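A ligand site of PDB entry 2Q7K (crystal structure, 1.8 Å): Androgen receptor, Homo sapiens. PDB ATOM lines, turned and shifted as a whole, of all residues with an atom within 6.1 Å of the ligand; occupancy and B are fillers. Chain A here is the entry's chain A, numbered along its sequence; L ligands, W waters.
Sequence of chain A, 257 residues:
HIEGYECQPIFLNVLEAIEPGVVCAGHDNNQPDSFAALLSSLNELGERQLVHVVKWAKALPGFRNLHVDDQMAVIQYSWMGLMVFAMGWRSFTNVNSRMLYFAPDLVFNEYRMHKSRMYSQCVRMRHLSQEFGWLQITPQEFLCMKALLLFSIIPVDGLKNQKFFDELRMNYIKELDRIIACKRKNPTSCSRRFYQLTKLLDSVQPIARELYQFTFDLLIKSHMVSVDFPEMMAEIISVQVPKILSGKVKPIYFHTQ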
ATOM      1  N   LEU A  39      -4.889   3.759   5.818  1.00  0.00           N
ATOM      2  CA  LEU A  39      -3.569   3.118   5.761  1.00  0.00           C
ATOM      3  C   LEU A  39      -3.458   1.939   6.707  1.00  0.00           C
ATOM      4  O   LEU A  39      -2.844   0.947   6.360  1.00  0.00           O
ATOM      5  CB  LEU A  39      -2.438   4.110   6.029  1.00  0.00           C
ATOM      6  CG  LEU A  39      -1.838   4.775   4.793  1.00  0.00           C
ATOM      7  CD1 LEU A  39      -1.133   3.729   3.923  1.00  0.00           C
ATOM      8  CD2 LEU A  39      -2.876   5.528   3.982  1.00  0.00           C
ATOM      9  N   LEU A  42      -5.202  -0.798   4.802  1.00  0.00           N
ATOM     10  CA  LEU A  42      -4.356  -1.311   3.724  1.00  0.00           C
ATOM     11  C   LEU A  42      -3.246  -2.191   4.285  1.00  0.00           C
ATOM     12  O   LEU A  42      -2.917  -3.246   3.697  1.00  0.00           O
ATOM     13  CB  LEU A  42      -3.762  -0.167   2.877  1.00  0.00           C
ATOM     14  CG  LEU A  42      -4.699   0.540   1.911  1.00  0.00           C
ATOM     15  CD1 LEU A  42      -4.009   1.795   1.394  1.00  0.00           C
ATOM     16  CD2 LEU A  42      -5.094  -0.388   0.741  1.00  0.00           C
ATOM     17  N   ASN A  43      -2.665  -1.789   5.403  1.00  0.00           N
ATOM     18  CA  ASN A  43      -1.611  -2.594   6.032  1.00  0.00           C
ATOM     19  C   ASN A  43      -2.111  -3.965   6.478  1.00  0.00           C
ATOM     20  O   ASN A  43      -1.446  -4.991   6.274  1.00  0.00           O
ATOM     21  CB  ASN A  43      -1.007  -1.848   7.229  1.00  0.00           C
ATOM     22  CG  ASN A  43      -0.149  -0.652   6.826  1.00  0.00           C
ATOM     23  OD1 ASN A  43       0.333  -0.559   5.679  1.00  0.00           O
ATOM     24  ND2 ASN A  43       0.086   0.254   7.775  1.00  0.00           N
ATOM     25  N   GLU A  44      -3.281  -3.979   7.095  1.00  0.00           N
ATOM     26  CA  GLU A  44      -3.903  -5.235   7.506  1.00  0.00           C
ATOM     27  C   GLU A  44      -4.206  -6.116   6.300  1.00  0.00           C
ATOM     28  O   GLU A  44      -3.982  -7.324   6.321  1.00  0.00           O
ATOM     29  CB  GLU A  44      -5.168  -4.968   8.309  1.00  0.00           C
ATOM     30  CG  GLU A  44      -5.952  -6.236   8.716  1.00  0.00           C
ATOM     31  CD  GLU A  44      -5.162  -7.222   9.571  1.00  0.00           C
ATOM     32  OE1 GLU A  44      -5.504  -8.425   9.550  1.00  0.00           O
ATOM     33  OE2 GLU A  44      -4.211  -6.800  10.267  1.00  0.00           O
ATOM     34  N   LEU A  45      -4.707  -5.499   5.234  1.00  0.00           N
ATOM     35  CA  LEU A  45      -4.960  -6.209   3.994  1.00  0.00           C
ATOM     36  C   LEU A  45      -3.686  -6.837   3.433  1.00  0.00           C
ATOM     37  O   LEU A  45      -3.686  -7.967   2.960  1.00  0.00           O
ATOM     38  CB  LEU A  45      -5.587  -5.263   2.952  1.00  0.00           C
ATOM     39  CG  LEU A  45      -5.911  -5.901   1.586  1.00  0.00           C
ATOM     40  CD1 LEU A  45      -6.949  -7.030   1.696  1.00  0.00           C
ATOM     41  CD2 LEU A  45      -6.365  -4.842   0.596  1.00  0.00           C
ATOM     42  N   GLY A  46      -2.596  -6.088   3.457  1.00  0.00           N
ATOM     43  CA  GLY A  46      -1.292  -6.632   3.051  1.00  0.00           C
ATOM     44  C   GLY A  46      -0.936  -7.858   3.865  1.00  0.00           C
ATOM     45  O   GLY A  46      -0.492  -8.855   3.312  1.00  0.00           O
ATOM     46  N   GLN A  49      -3.185 -10.715   2.687  1.00  0.00           N
ATOM     47  CA  GLN A  49      -2.822 -11.143   1.333  1.00  0.00           C
ATOM     48  C   GLN A  49      -1.496 -11.883   1.308  1.00  0.00           C
ATOM     49  O   GLN A  49      -1.322 -12.785   0.491  1.00  0.00           O
ATOM     50  CB  GLN A  49      -2.827  -9.968   0.360  1.00  0.00           C
ATOM     51  CG  GLN A  49      -4.236  -9.515  -0.037  1.00  0.00           C
ATOM     52  CD  GLN A  49      -4.277  -8.613  -1.250  1.00  0.00           C
ATOM     53  OE1 GLN A  49      -5.316  -8.018  -1.549  1.00  0.00           O
ATOM     54  NE2 GLN A  49      -3.170  -8.510  -1.959  1.00  0.00           N
ATOM     55  N   TRP A  79       6.385  -9.361  -3.350  1.00  0.00           N
ATOM     56  CA  TRP A  79       5.002  -9.250  -2.883  1.00  0.00           C
ATOM     57  C   TRP A  79       4.293  -7.962  -3.313  1.00  0.00           C
ATOM     58  O   TRP A  79       3.138  -7.995  -3.696  1.00  0.00           O
ATOM     59  CB  TRP A  79       4.891  -9.432  -1.354  1.00  0.00           C
ATOM     60  CG  TRP A  79       5.626  -8.402  -0.561  1.00  0.00           C
ATOM     61  CD1 TRP A  79       6.935  -8.418  -0.245  1.00  0.00           C
ATOM     62  CD2 TRP A  79       5.070  -7.233   0.048  1.00  0.00           C
ATOM     63  NE1 TRP A  79       7.262  -7.326   0.499  1.00  0.00           N
ATOM     64  CE2 TRP A  79       6.133  -6.574   0.709  1.00  0.00           C
ATOM     65  CE3 TRP A  79       3.795  -6.663   0.092  1.00  0.00           C
ATOM     66  CZ2 TRP A  79       5.953  -5.381   1.395  1.00  0.00           C
ATOM     67  CZ3 TRP A  79       3.617  -5.484   0.775  1.00  0.00           C
ATOM     68  CH2 TRP A  79       4.683  -4.853   1.431  1.00  0.00           C
ATOM     69  N   MET A  80       4.986  -6.824  -3.261  1.00  0.00           N
ATOM     70  CA  MET A  80       4.331  -5.552  -3.604  1.00  0.00           C
ATOM     71  C   MET A  80       3.863  -5.562  -5.056  1.00  0.00           C
ATOM     72  O   MET A  80       2.714  -5.226  -5.355  1.00  0.00           O
ATOM     73  CB  MET A  80       5.258  -4.358  -3.351  1.00  0.00           C
ATOM     74  CG  MET A  80       4.605  -3.020  -3.622  1.00  0.00           C
ATOM     75  SD  MET A  80       3.382  -2.535  -2.397  1.00  0.00           S
ATOM     76  CE  MET A  80       4.482  -2.124  -1.060  1.00  0.00           C
ATOM     77  N   MET A  83       0.977  -8.036  -5.616  1.00  0.00           N
ATOM     78  CA  MET A  83      -0.300  -7.561  -5.051  1.00  0.00           C
ATOM     79  C   MET A  83      -0.884  -6.388  -5.842  1.00  0.00           C
ATOM     80  O   MET A  83      -2.104  -6.306  -6.029  1.00  0.00           O
ATOM     81  CB  MET A  83      -0.105  -7.182  -3.581  1.00  0.00           C
ATOM     82  CG  MET A  83       0.160  -8.401  -2.670  1.00  0.00           C
ATOM     83  SD  MET A  83       0.321  -7.976  -0.957  1.00  0.00           S
ATOM     84  CE  MET A  83       0.865  -9.538  -0.282  1.00  0.00           C
ATOM     85  N   VAL A  84      -0.019  -5.485  -6.297  1.00  0.00           N
ATOM     86  CA  VAL A  84      -0.457  -4.348  -7.112  1.00  0.00           C
ATOM     87  C   VAL A  84      -1.034  -4.828  -8.438  1.00  0.00           C
ATOM     88  O   VAL A  84      -2.094  -4.379  -8.864  1.00  0.00           O
ATOM     89  CB  VAL A  84       0.701  -3.348  -7.352  1.00  0.00           C
ATOM     90  CG1 VAL A  84       0.319  -2.310  -8.421  1.00  0.00           C
ATOM     91  CG2 VAL A  84       1.093  -2.648  -6.081  1.00  0.00           C
ATOM     92  N   MET A  87      -4.332  -6.430  -7.899  1.00  0.00           N
ATOM     93  CA  MET A  87      -5.301  -5.387  -7.544  1.00  0.00           C
ATOM     94  C   MET A  87      -5.716  -4.644  -8.806  1.00  0.00           C
ATOM     95  O   MET A  87      -6.893  -4.340  -8.987  1.00  0.00           O
ATOM     96  CB  MET A  87      -4.728  -4.429  -6.501  1.00  0.00           C
ATOM     97  CG  MET A  87      -5.718  -3.406  -5.976  1.00  0.00           C
ATOM     98  SD  MET A  87      -5.881  -1.946  -6.993  1.00  0.00           S
ATOM     99  CE  MET A  87      -4.247  -1.226  -6.808  1.00  0.00           C
ATOM    100  N   ARG A  90      -8.218  -6.859 -10.499  1.00  0.00           N
ATOM    101  CA  ARG A  90      -9.533  -6.793  -9.820  1.00  0.00           C
ATOM    102  C   ARG A  90     -10.273  -5.520 -10.149  1.00  0.00           C
ATOM    103  O   ARG A  90     -11.495  -5.539 -10.334  1.00  0.00           O
ATOM    104  CB  ARG A  90      -9.381  -6.851  -8.283  1.00  0.00           C
ATOM    105  CG  ARG A  90      -8.935  -8.177  -7.735  1.00  0.00           C
ATOM    106  CD  ARG A  90      -9.133  -8.235  -6.231  1.00  0.00           C
ATOM    107  NE  ARG A  90      -8.285  -7.317  -5.463  1.00  0.00           N
ATOM    108  CZ  ARG A  90      -6.995  -7.532  -5.180  1.00  0.00           C
ATOM    109  NH1 ARG A  90      -6.371  -8.624  -5.607  1.00  0.00           N
ATOM    110  NH2 ARG A  90      -6.335  -6.652  -4.450  1.00  0.00           N
ATOM    111  N   TYR A 101      -9.848  -1.315  -6.598  1.00  0.00           N
ATOM    112  CA  TYR A 101     -10.521  -2.370  -5.854  1.00  0.00           C
ATOM    113  C   TYR A 101      -9.522  -3.139  -4.982  1.00  0.00           C
ATOM    114  O   TYR A 101      -9.172  -4.289  -5.273  1.00  0.00           O
ATOM    115  CB  TYR A 101     -11.209  -3.308  -6.847  1.00  0.00           C
ATOM    116  CG  TYR A 101     -12.336  -4.145  -6.285  1.00  0.00           C
ATOM    117  CD1 TYR A 101     -13.665  -3.743  -6.391  1.00  0.00           C
ATOM    118  CD2 TYR A 101     -12.079  -5.366  -5.689  1.00  0.00           C
ATOM    119  CE1 TYR A 101     -14.700  -4.531  -5.886  1.00  0.00           C
ATOM    120  CE2 TYR A 101     -13.092  -6.158  -5.186  1.00  0.00           C
ATOM    121  CZ  TYR A 101     -14.403  -5.732  -5.288  1.00  0.00           C
ATOM    122  OH  TYR A 101     -15.406  -6.544  -4.790  1.00  0.00           O
ATOM    123  N   PHE A 102      -9.064  -2.504  -3.909  1.00  0.00           N
ATOM    124  CA  PHE A 102      -8.112  -3.176  -3.008  1.00  0.00           C
ATOM    125  C   PHE A 102      -8.735  -4.440  -2.435  1.00  0.00           C
ATOM    126  O   PHE A 102      -8.095  -5.486  -2.346  1.00  0.00           O
ATOM    127  CB  PHE A 102      -7.648  -2.242  -1.902  1.00  0.00           C
ATOM    128  CG  PHE A 102      -6.714  -1.162  -2.371  1.00  0.00           C
ATOM    129  CD1 PHE A 102      -5.380  -1.452  -2.642  1.00  0.00           C
ATOM    130  CD2 PHE A 102      -7.151   0.131  -2.528  1.00  0.00           C
ATOM    131  CE1 PHE A 102      -4.505  -0.458  -3.072  1.00  0.00           C
ATOM    132  CE2 PHE A 102      -6.298   1.129  -2.956  1.00  0.00           C
ATOM    133  CZ  PHE A 102      -4.971   0.831  -3.229  1.00  0.00           C
ATOM    134  N   ALA A 103     -10.008  -4.327  -2.065  1.00  0.00           N
ATOM    135  CA  ALA A 103     -10.779  -5.443  -1.530  1.00  0.00           C
ATOM    136  C   ALA A 103     -12.252  -5.084  -1.615  1.00  0.00           C
ATOM    137  O   ALA A 103     -12.571  -3.912  -1.861  1.00  0.00           O
ATOM    138  CB  ALA A 103     -10.383  -5.705  -0.102  1.00  0.00           C
ATOM    139  N   MET A 118      -1.513   9.170  -1.071  1.00  0.00           N
ATOM    140  CA  MET A 118      -0.851   8.328  -2.055  1.00  0.00           C
ATOM    141  C   MET A 118      -1.449   8.565  -3.437  1.00  0.00           C
ATOM    142  O   MET A 118      -1.487   7.652  -4.256  1.00  0.00           O
ATOM    143  CB  MET A 118      -1.004   6.848  -1.697  1.00  0.00           C
ATOM    144  CG  MET A 118      -0.376   6.458  -0.405  1.00  0.00           C
ATOM    145  SD  MET A 118      -0.226   4.683  -0.215  1.00  0.00           S
ATOM    146  CE  MET A 118      -1.953   4.207  -0.129  1.00  0.00           C
ATOM    147  N   MET A 125      -1.287   3.211 -10.401  1.00  0.00           N
ATOM    148  CA  MET A 125      -1.978   1.921 -10.287  1.00  0.00           C
ATOM    149  C   MET A 125      -3.249   1.861 -11.117  1.00  0.00           C
ATOM    150  O   MET A 125      -3.547   0.847 -11.747  1.00  0.00           O
ATOM    151  CB  MET A 125      -2.278   1.591  -8.825  1.00  0.00           C
ATOM    152  CG  MET A 125      -1.013   1.299  -8.016  1.00  0.00           C
ATOM    153  SD  MET A 125      -1.299   0.662  -6.364  1.00  0.00           S
ATOM    154  CE  MET A 125      -1.764   2.134  -5.493  1.00  0.00           C
ATOM    155  N   LEU A 211       5.794   2.638  -4.023  1.00  0.00           N
ATOM    156  CA  LEU A 211       5.024   2.171  -2.876  1.00  0.00           C
ATOM    157  C   LEU A 211       5.925   1.675  -1.739  1.00  0.00           C
ATOM    158  O   LEU A 211       5.631   1.904  -0.565  1.00  0.00           O
ATOM    159  CB  LEU A 211       4.057   1.074  -3.334  1.00  0.00           C
ATOM    160  CG  LEU A 211       2.912   1.586  -4.202  1.00  0.00           C
ATOM    161  CD1 LEU A 211       2.207   0.454  -4.893  1.00  0.00           C
ATOM    162  CD2 LEU A 211       1.921   2.413  -3.356  1.00  0.00           C
ATOM    163  N   PHE A 214       7.200   4.757  -0.013  1.00  0.00           N
ATOM    164  CA  PHE A 214       6.108   5.339   0.764  1.00  0.00           C
ATOM    165  C   PHE A 214       5.838   4.559   2.055  1.00  0.00           C
ATOM    166  O   PHE A 214       5.690   5.133   3.139  1.00  0.00           O
ATOM    167  CB  PHE A 214       4.839   5.433  -0.079  1.00  0.00           C
ATOM    168  CG  PHE A 214       3.699   6.100   0.635  1.00  0.00           C
ATOM    169  CD1 PHE A 214       2.845   5.373   1.446  1.00  0.00           C
ATOM    170  CD2 PHE A 214       3.480   7.473   0.500  1.00  0.00           C
ATOM    171  CE1 PHE A 214       1.788   5.995   2.107  1.00  0.00           C
ATOM    172  CE2 PHE A 214       2.432   8.087   1.170  1.00  0.00           C
ATOM    173  CZ  PHE A 214       1.592   7.349   1.968  1.00  0.00           C
ATOM    174  N   THR A 215       5.758   3.237   1.949  1.00  0.00           N
ATOM    175  CA  THR A 215       5.452   2.424   3.113  1.00  0.00           C
ATOM    176  C   THR A 215       6.627   2.386   4.104  1.00  0.00           C
ATOM    177  O   THR A 215       6.407   2.372   5.312  1.00  0.00           O
ATOM    178  CB  THR A 215       4.979   0.991   2.724  1.00  0.00           C
ATOM    179  OG1 THR A 215       4.269   0.430   3.831  1.00  0.00           O
ATOM    180  CG2 THR A 215       6.144   0.079   2.342  1.00  0.00           C
ATOM    181  N   LEU A 218       6.522   5.583   5.960  1.00  0.00           N
ATOM    182  CA  LEU A 218       5.369   5.544   6.846  1.00  0.00           C
ATOM    183  C   LEU A 218       5.646   4.710   8.078  1.00  0.00           C
ATOM    184  O   LEU A 218       5.281   5.093   9.191  1.00  0.00           O
ATOM    185  CB  LEU A 218       4.145   5.012   6.094  1.00  0.00           C
ATOM    186  CG  LEU A 218       2.824   4.983   6.858  1.00  0.00           C
ATOM    187  CD1 LEU A 218       2.509   6.336   7.527  1.00  0.00           C
ATOM    188  CD2 LEU A 218       1.732   4.594   5.880  1.00  0.00           C
ATOM    189  N   PHE A 229       0.947  -1.009  11.800  1.00  0.00           N
ATOM    190  CA  PHE A 229       1.549  -2.036  10.918  1.00  0.00           C
ATOM    191  C   PHE A 229       1.490  -3.393  11.619  1.00  0.00           C
ATOM    192  O   PHE A 229       2.018  -3.538  12.725  1.00  0.00           O
ATOM    193  CB  PHE A 229       3.002  -1.707  10.586  1.00  0.00           C
ATOM    194  CG  PHE A 229       3.168  -0.667   9.510  1.00  0.00           C
ATOM    195  CD1 PHE A 229       3.057   0.690   9.814  1.00  0.00           C
ATOM    196  CD2 PHE A 229       3.433  -1.035   8.202  1.00  0.00           C
ATOM    197  CE1 PHE A 229       3.206   1.654   8.827  1.00  0.00           C
ATOM    198  CE2 PHE A 229       3.590  -0.075   7.203  1.00  0.00           C
ATOM    199  CZ  PHE A 229       3.472   1.272   7.516  1.00  0.00           C
ATOM    200  N   MET A 233       4.188  -7.414   8.123  1.00  0.00           N
ATOM    201  CA  MET A 233       4.434  -6.207   7.336  1.00  0.00           C
ATOM    202  C   MET A 233       5.575  -5.383   7.940  1.00  0.00           C
ATOM    203  O   MET A 233       6.484  -5.009   7.237  1.00  0.00           O
ATOM    204  CB  MET A 233       3.156  -5.377   7.181  1.00  0.00           C
ATOM    205  CG  MET A 233       2.114  -6.033   6.275  1.00  0.00           C
ATOM    206  SD  MET A 233       2.494  -5.892   4.512  1.00  0.00           S
ATOM    207  CE  MET A 233       2.030  -4.191   4.244  1.00  0.00           C
ATOM    208  N   ILE A 237       9.018  -4.880   5.931  1.00  0.00           N
ATOM    209  CA  ILE A 237       9.290  -3.511   5.506  1.00  0.00           C
ATOM    210  C   ILE A 237      10.603  -2.982   6.131  1.00  0.00           C
ATOM    211  O   ILE A 237      11.280  -2.153   5.520  1.00  0.00           O
ATOM    212  CB  ILE A 237       8.081  -2.572   5.753  1.00  0.00           C
ATOM    213  CG1 ILE A 237       6.924  -2.993   4.833  1.00  0.00           C
ATOM    214  CG2 ILE A 237       8.461  -1.119   5.490  1.00  0.00           C
ATOM    215  CD1 ILE A 237       5.605  -2.404   5.177  1.00  0.00           C
HETATM  216  C1  LIG L   1      -2.361  -4.287  -0.051  1.00  0.00           C
HETATM  217  C2  LIG L   1      -2.942  -5.329  -0.997  1.00  0.00           C
HETATM  218  C3  LIG L   1      -3.264  -4.726  -2.338  1.00  0.00           C
HETATM  219  O1  LIG L   1      -4.213  -5.157  -2.985  1.00  0.00           O
HETATM  220  C4  LIG L   1      -2.479  -3.600  -2.842  1.00  0.00           C
HETATM  221  C5  LIG L   1      -1.538  -3.025  -2.078  1.00  0.00           C
HETATM  222  C6  LIG L   1      -0.773  -1.869  -2.677  1.00  0.00           C
HETATM  223  C7  LIG L   1      -0.614  -0.743  -1.675  1.00  0.00           C
HETATM  224  C8  LIG L   1       0.013  -1.236  -0.380  1.00  0.00           C
HETATM  225  C9  LIG L   1      -0.866  -2.318   0.258  1.00  0.00           C
HETATM  226  C10 LIG L   1      -1.187  -3.505  -0.676  1.00  0.00           C
HETATM  227  C11 LIG L   1      -0.293  -2.763   1.614  1.00  0.00           C
HETATM  228  C12 LIG L   1      -0.106  -1.590   2.573  1.00  0.00           C
HETATM  229  C13 LIG L   1       0.783  -0.519   1.963  1.00  0.00           C
HETATM  230  C14 LIG L   1       0.183  -0.081   0.627  1.00  0.00           C
HETATM  231  C15 LIG L   1       1.017   1.141   0.269  1.00  0.00           C
HETATM  232  C16 LIG L   1       1.227   1.831   1.630  1.00  0.00           C
HETATM  233  C17 LIG L   1       0.809   0.812   2.703  1.00  0.00           C
HETATM  234  O2  LIG L   1       1.702   0.825   3.818  1.00  0.00           O
HETATM  235  C18 LIG L   1       2.219  -1.036   1.819  1.00  0.00           C
HETATM  236  C19 LIG L   1       0.003  -4.451  -0.852  1.00  0.00           C
HETATM  237  O   HOH W   1      -3.658  -8.000  -4.498  1.00  0.00           O
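The side-chain hydroxyl of Thr 215 lies within hydrogen-bond range of an oxygen (O2) of the ligand.
O2 of the ligand is in hydrogen-bond range of OD1 of Asn 43 (2.7 Å).
The guanidinium group (NH2) of Arg 90 lies within hydrogen-bond range of an oxygen (O1) of the ligand (3.0 Å).
An oxygen (O1) of the ligand lies close to the side-chain amide oxygen (OE1) of Gln 49 (3.4 Å).
The backbone carbonyl oxygen of Leu 39 sits close to the side-chain amide nitrogen of Asn 43.
The side-chain amide oxygen (OE1) of Gln 49 lies within hydrogen-bond range of the guanidinium group (NH2) of Arg 90 (3.4 Å).
NH2 of Arg 90 is in hydrogen-bond range of O of Phe 102, 3.0 Å away.
The backbone carbonyl oxygen of Tyr 101 lies within hydrogen-bond range of the guanidinium group of Arg 90 (3.2 Å).
NE2 of Gln 49 sits close to SD of Met 83 (3.7 Å).
Residues that only touch the ligand: Leu 42, Met 83, Phe 102, Met 87, Met 118, Leu 39, Met 233, Leu 45, Met 80, Phe 214, Leu 211, Gly 46, Val 84 and Phe 229.
Hydrophobic or aromatic side chains within 4 Å of the ligand: Leu 39, Leu 42, Leu 45, Met 80, Met 83, Val 84, Met 87, Phe 102, Met 118, Leu 211, Phe 214, Phe 229 and Met 233.
Within 4 Å of the ligand: Leu 39, Leu 42, Asn 43, Leu 45, Gly 46, Gln 49, Met 80, Met 83, Val 84, Met 87, Arg 90, Phe 102, Met 118, Leu 211, Phe 214, Thr 215, Phe 229 and Met 233.
The nearest printed residue that does not touch the ligand is Trp 79 (4.1 Å).
Water W1 lies within hydrogen-bond range of NE2 of Gln 49, O of Met 83, NH1 of Arg 90 and O1 of the ligand.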
